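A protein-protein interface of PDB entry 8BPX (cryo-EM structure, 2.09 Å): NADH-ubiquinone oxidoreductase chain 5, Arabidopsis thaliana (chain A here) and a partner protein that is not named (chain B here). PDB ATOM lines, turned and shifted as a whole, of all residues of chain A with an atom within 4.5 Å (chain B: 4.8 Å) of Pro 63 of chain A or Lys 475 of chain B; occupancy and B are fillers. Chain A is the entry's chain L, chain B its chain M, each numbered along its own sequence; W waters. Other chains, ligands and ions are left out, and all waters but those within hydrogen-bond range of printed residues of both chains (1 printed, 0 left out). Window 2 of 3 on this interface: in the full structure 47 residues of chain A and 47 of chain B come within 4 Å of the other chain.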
ATOM      1  N   ARG A  60      31.834 -26.361   7.918  1.00  0.00           N
ATOM      2  CA  ARG A  60      30.445 -26.211   8.332  1.00  0.00           C
ATOM      3  C   ARG A  60      30.374 -26.380   9.844  1.00  0.00           C
ATOM      4  O   ARG A  60      30.731 -27.435  10.375  1.00  0.00           O
ATOM      5  CB  ARG A  60      29.549 -27.217   7.609  1.00  0.00           C
ATOM      6  CG  ARG A  60      28.074 -26.942   7.802  1.00  0.00           C
ATOM      7  CD  ARG A  60      27.222 -28.175   7.617  1.00  0.00           C
ATOM      8  NE  ARG A  60      25.806 -27.838   7.685  1.00  0.00           N
ATOM      9  CZ  ARG A  60      25.059 -27.972   8.771  1.00  0.00           C
ATOM     10  NH1 ARG A  60      25.552 -28.475   9.889  1.00  0.00           N
ATOM     11  NH2 ARG A  60      23.786 -27.592   8.735  1.00  0.00           N
ATOM     12  N   ALA A  62      27.416 -25.478  12.053  1.00  0.00           N
ATOM     13  CA  ALA A  62      26.115 -25.928  12.521  1.00  0.00           C
ATOM     14  C   ALA A  62      25.047 -25.339  11.607  1.00  0.00           C
ATOM     15  O   ALA A  62      25.304 -24.356  10.911  1.00  0.00           O
ATOM     16  CB  ALA A  62      25.866 -25.505  13.980  1.00  0.00           C
ATOM     17  N   PRO A  63      23.855 -25.934  11.584  1.00  0.00           N
ATOM     18  CA  PRO A  63      22.727 -25.274  10.920  1.00  0.00           C
ATOM     19  C   PRO A  63      22.376 -23.977  11.629  1.00  0.00           C
ATOM     20  O   PRO A  63      22.440 -23.881  12.854  1.00  0.00           O
ATOM     21  CB  PRO A  63      21.593 -26.297  11.044  1.00  0.00           C
ATOM     22  CG  PRO A  63      21.963 -27.114  12.235  1.00  0.00           C
ATOM     23  CD  PRO A  63      23.455 -27.207  12.207  1.00  0.00           C
ATOM     24  N   TRP A  64      22.026 -22.963  10.843  1.00  0.00           N
ATOM     25  CA  TRP A  64      21.489 -21.726  11.395  1.00  0.00           C
ATOM     26  C   TRP A  64      19.964 -21.704  11.333  1.00  0.00           C
ATOM     27  O   TRP A  64      19.302 -21.698  12.370  1.00  0.00           O
ATOM     28  CB  TRP A  64      22.094 -20.524  10.664  1.00  0.00           C
ATOM     29  CG  TRP A  64      21.639 -19.191  11.178  1.00  0.00           C
ATOM     30  CD1 TRP A  64      21.028 -18.931  12.368  1.00  0.00           C
ATOM     31  CD2 TRP A  64      21.743 -17.938  10.499  1.00  0.00           C
ATOM     32  NE1 TRP A  64      20.752 -17.595  12.476  1.00  0.00           N
ATOM     33  CE2 TRP A  64      21.181 -16.961  11.343  1.00  0.00           C
ATOM     34  CE3 TRP A  64      22.262 -17.545   9.262  1.00  0.00           C
ATOM     35  CZ2 TRP A  64      21.118 -15.618  10.987  1.00  0.00           C
ATOM     36  CZ3 TRP A  64      22.204 -16.214   8.912  1.00  0.00           C
ATOM     37  CH2 TRP A  64      21.634 -15.265   9.771  1.00  0.00           C
ATOM     38  N   ILE A  65      19.397 -21.738  10.133  1.00  0.00           N
ATOM     39  CA  ILE A  65      17.952 -21.691   9.941  1.00  0.00           C
ATOM     40  C   ILE A  65      17.566 -22.883   9.080  1.00  0.00           C
ATOM     41  O   ILE A  65      17.806 -22.885   7.868  1.00  0.00           O
ATOM     42  CB  ILE A  65      17.490 -20.375   9.298  1.00  0.00           C
ATOM     43  CG1 ILE A  65      17.995 -19.182  10.114  1.00  0.00           C
ATOM     44  CG2 ILE A  65      15.972 -20.345   9.186  1.00  0.00           C
ATOM     45  CD1 ILE A  65      18.447 -18.010   9.284  1.00  0.00           C
ATOM     46  N   ALA A  72      19.734 -22.473   5.555  1.00  0.00           N
ATOM     47  CA  ALA A  72      20.778 -21.542   5.969  1.00  0.00           C
ATOM     48  C   ALA A  72      21.616 -22.157   7.085  1.00  0.00           C
ATOM     49  O   ALA A  72      21.087 -22.771   8.013  1.00  0.00           O
ATOM     50  CB  ALA A  72      20.164 -20.223   6.430  1.00  0.00           C
ATOM     51  N   SER A  73      22.933 -21.994   6.990  1.00  0.00           N
ATOM     52  CA  SER A  73      23.844 -22.638   7.926  1.00  0.00           C
ATOM     53  C   SER A  73      24.984 -21.697   8.289  1.00  0.00           C
ATOM     54  O   SER A  73      25.263 -20.722   7.593  1.00  0.00           O
ATOM     55  CB  SER A  73      24.402 -23.943   7.347  1.00  0.00           C
ATOM     56  OG  SER A  73      25.188 -23.694   6.200  1.00  0.00           O
ATOM     57  N   TRP A  74      25.629 -21.996   9.417  1.00  0.00           N
ATOM     58  CA  TRP A  74      26.890 -21.363   9.794  1.00  0.00           C
ATOM     59  C   TRP A  74      28.002 -22.130   9.087  1.00  0.00           C
ATOM     60  O   TRP A  74      28.548 -23.099   9.610  1.00  0.00           O
ATOM     61  CB  TRP A  74      27.078 -21.364  11.307  1.00  0.00           C
ATOM     62  CG  TRP A  74      26.035 -20.592  12.044  1.00  0.00           C
ATOM     63  CD1 TRP A  74      25.057 -21.097  12.847  1.00  0.00           C
ATOM     64  CD2 TRP A  74      25.847 -19.175  12.026  1.00  0.00           C
ATOM     65  NE1 TRP A  74      24.277 -20.084  13.335  1.00  0.00           N
ATOM     66  CE2 TRP A  74      24.738 -18.892  12.847  1.00  0.00           C
ATOM     67  CE3 TRP A  74      26.510 -18.118  11.397  1.00  0.00           C
ATOM     68  CZ2 TRP A  74      24.279 -17.597  13.060  1.00  0.00           C
ATOM     69  CZ3 TRP A  74      26.052 -16.833  11.608  1.00  0.00           C
ATOM     70  CH2 TRP A  74      24.945 -16.583  12.436  1.00  0.00           C
ATOM     71  N   VAL B 472      20.633 -17.130  17.020  1.00  0.00           N
ATOM     72  CA  VAL B 472      21.767 -17.845  16.437  1.00  0.00           C
ATOM     73  C   VAL B 472      21.460 -19.328  16.252  1.00  0.00           C
ATOM     74  O   VAL B 472      21.978 -19.957  15.326  1.00  0.00           O
ATOM     75  CB  VAL B 472      23.058 -17.647  17.259  1.00  0.00           C
ATOM     76  CG1 VAL B 472      23.389 -16.170  17.379  1.00  0.00           C
ATOM     77  CG2 VAL B 472      22.973 -18.319  18.627  1.00  0.00           C
ATOM     78  N   TYR B 473      20.626 -19.900  17.113  1.00  0.00           N
ATOM     79  CA  TYR B 473      20.298 -21.325  17.049  1.00  0.00           C
ATOM     80  C   TYR B 473      18.801 -21.541  17.241  1.00  0.00           C
ATOM     81  O   TYR B 473      18.364 -22.134  18.231  1.00  0.00           O
ATOM     82  CB  TYR B 473      21.105 -22.109  18.085  1.00  0.00           C
ATOM     83  CG  TYR B 473      21.306 -23.556  17.714  1.00  0.00           C
ATOM     84  CD1 TYR B 473      21.968 -23.906  16.544  1.00  0.00           C
ATOM     85  CD2 TYR B 473      20.816 -24.573  18.519  1.00  0.00           C
ATOM     86  CE1 TYR B 473      22.148 -25.224  16.193  1.00  0.00           C
ATOM     87  CE2 TYR B 473      20.995 -25.898  18.180  1.00  0.00           C
ATOM     88  CZ  TYR B 473      21.662 -26.219  17.011  1.00  0.00           C
ATOM     89  OH  TYR B 473      21.838 -27.533  16.657  1.00  0.00           O
ATOM     90  N   PRO B 474      17.980 -21.102  16.281  1.00  0.00           N
ATOM     91  CA  PRO B 474      16.531 -21.331  16.395  1.00  0.00           C
ATOM     92  C   PRO B 474      16.117 -22.785  16.222  1.00  0.00           C
ATOM     93  O   PRO B 474      14.919 -23.077  16.274  1.00  0.00           O
ATOM     94  CB  PRO B 474      15.955 -20.451  15.278  1.00  0.00           C
ATOM     95  CG  PRO B 474      17.043 -20.364  14.280  1.00  0.00           C
ATOM     96  CD  PRO B 474      18.323 -20.364  15.053  1.00  0.00           C
ATOM     97  N   LYS B 475      17.070 -23.703  16.042  1.00  0.00           N
ATOM     98  CA  LYS B 475      16.738 -25.108  15.841  1.00  0.00           C
ATOM     99  C   LYS B 475      16.065 -25.722  17.064  1.00  0.00           C
ATOM    100  O   LYS B 475      15.185 -26.573  16.910  1.00  0.00           O
ATOM    101  CB  LYS B 475      17.999 -25.895  15.479  1.00  0.00           C
ATOM    102  CG  LYS B 475      17.766 -27.375  15.249  1.00  0.00           C
ATOM    103  CD  LYS B 475      18.986 -28.041  14.629  1.00  0.00           C
ATOM    104  CE  LYS B 475      18.905 -29.559  14.731  1.00  0.00           C
ATOM    105  NZ  LYS B 475      18.832 -30.016  16.139  1.00  0.00           N
ATOM    106  N   VAL B 476      16.450 -25.305  18.276  1.00  0.00           N
ATOM    107  CA  VAL B 476      15.829 -25.864  19.479  1.00  0.00           C
ATOM    108  C   VAL B 476      14.325 -25.635  19.464  1.00  0.00           C
ATOM    109  O   VAL B 476      13.550 -26.502  19.885  1.00  0.00           O
ATOM    110  CB  VAL B 476      16.468 -25.289  20.759  1.00  0.00           C
ATOM    111  CG1 VAL B 476      17.723 -26.036  21.096  1.00  0.00           C
ATOM    112  CG2 VAL B 476      16.730 -23.792  20.632  1.00  0.00           C
ATOM    113  N   PHE B 477      13.889 -24.473  18.984  1.00  0.00           N
ATOM    114  CA  PHE B 477      12.461 -24.188  18.919  1.00  0.00           C
ATOM    115  C   PHE B 477      11.804 -24.856  17.715  1.00  0.00           C
ATOM    116  O   PHE B 477      10.750 -25.484  17.847  1.00  0.00           O
ATOM    117  CB  PHE B 477      12.239 -22.675  18.904  1.00  0.00           C
ATOM    118  CG  PHE B 477      12.808 -21.979  20.105  1.00  0.00           C
ATOM    119  CD1 PHE B 477      12.086 -21.906  21.284  1.00  0.00           C
ATOM    120  CD2 PHE B 477      14.077 -21.426  20.067  1.00  0.00           C
ATOM    121  CE1 PHE B 477      12.612 -21.278  22.397  1.00  0.00           C
ATOM    122  CE2 PHE B 477      14.607 -20.799  21.174  1.00  0.00           C
ATOM    123  CZ  PHE B 477      13.874 -20.727  22.344  1.00  0.00           C
ATOM    124  N   LEU B 478      12.424 -24.748  16.538  1.00  0.00           N
ATOM    125  CA  LEU B 478      11.797 -25.250  15.318  1.00  0.00           C
ATOM    126  C   LEU B 478      11.680 -26.772  15.312  1.00  0.00           C
ATOM    127  O   LEU B 478      10.750 -27.315  14.708  1.00  0.00           O
ATOM    128  CB  LEU B 478      12.575 -24.760  14.095  1.00  0.00           C
ATOM    129  CG  LEU B 478      12.393 -23.277  13.758  1.00  0.00           C
ATOM    130  CD1 LEU B 478      13.258 -22.858  12.586  1.00  0.00           C
ATOM    131  CD2 LEU B 478      10.925 -22.942  13.495  1.00  0.00           C
ATOM    132  N   ASP B 479      12.601 -27.474  15.978  1.00  0.00           N
ATOM    133  CA  ASP B 479      12.532 -28.930  16.032  1.00  0.00           C
ATOM    134  C   ASP B 479      11.317 -29.410  16.818  1.00  0.00           C
ATOM    135  O   ASP B 479      10.707 -30.420  16.455  1.00  0.00           O
ATOM    136  CB  ASP B 479      13.811 -29.496  16.644  1.00  0.00           C
ATOM    137  CG  ASP B 479      14.919 -29.677  15.625  1.00  0.00           C
ATOM    138  OD1 ASP B 479      15.949 -30.285  15.978  1.00  0.00           O
ATOM    139  OD2 ASP B 479      14.763 -29.217  14.477  1.00  0.00           O
HETATM  140  O   HOH W   1      19.690 -23.239  14.289  1.00  0.00           O
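The indole nitrogen (NE1) of Trp 74 of chain A is in hydrogen-bond range of the backbone carbonyl oxygen (O) of Val 472 of chain B, at 3.0 Å.
NZ of Lys 475 of chain B lies within salt-bridge range of OD1 of Asp 479 of chain B (2.9 Å).
N of Trp 74 of chain A sits at hydrogen-bond distance from O of Ala 62 of chain A, at 2.8 Å.
N of Trp 64 of chain A is in hydrogen-bond range of O of Ala 72 of chain A.
Among the printed residues, merely in contact across the chains: Pro 63 of chain A with Tyr 473 of chain B, Pro 63 of chain A with Lys 475 of chain B, Trp 64 of chain A with Val 472 of chain B and Trp 64 of chain A with Pro 474 of chain B.
Printed residues of chain B within 4 Å of Pro 63 of chain A: Tyr 473 (3.6 Å) and Lys 475 (3.9 Å).
Of the printed residues of chain B, Trp 64 of chain A touches Val 472 and Pro 474.
Ala 72 of chain A touches none of the printed residues of chain B.
Printed residues of chain B within 4 Å of Trp 74 of chain A: Val 472.
Printed residues of chain A within 4 Å of Val 472 of chain B: Trp 64 and Trp 74.
Of the printed residues of chain A, Tyr 473 of chain B touches Pro 63.
Of the printed residues of chain A, Pro 474 of chain B touches Trp 64.
Lys 475 of chain B touches one residue of chain A.
The nearest residue of chain B that does not touch Pro 63 of chain A is Val 472 of chain B (4.7 Å).
The nearest printed residue of chain A that does not touch Lys 475 of chain B is Trp 64 of chain A (4.7 Å).
The nearest printed residue of chain B that does not touch Trp 64 of chain A is Lys 475 of chain B (4.7 Å).
Of the 8 printed residues of chain A, 3 touch a printed residue of chain B.
Hydrophobic or aromatic side chains of chain A that line the printed part of chain B: Pro 63, Trp 64 and Trp 74.
Hydrophobic or aromatic side chains of chain B within 4 Å of the printed part of chain A: Tyr 473 and Pro 474.
Among the printed residues, no Asp or Glu carboxylate lies within 4 Å of a Lys or Arg side-chain nitrogen of the other chain.
Water W1 lies within hydrogen-bond range of O of Trp 64 of chain A (2.5 Å), O of Pro 63 of chain A (3.2 Å) and N of Lys 475 of chain B (3.2 Å).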
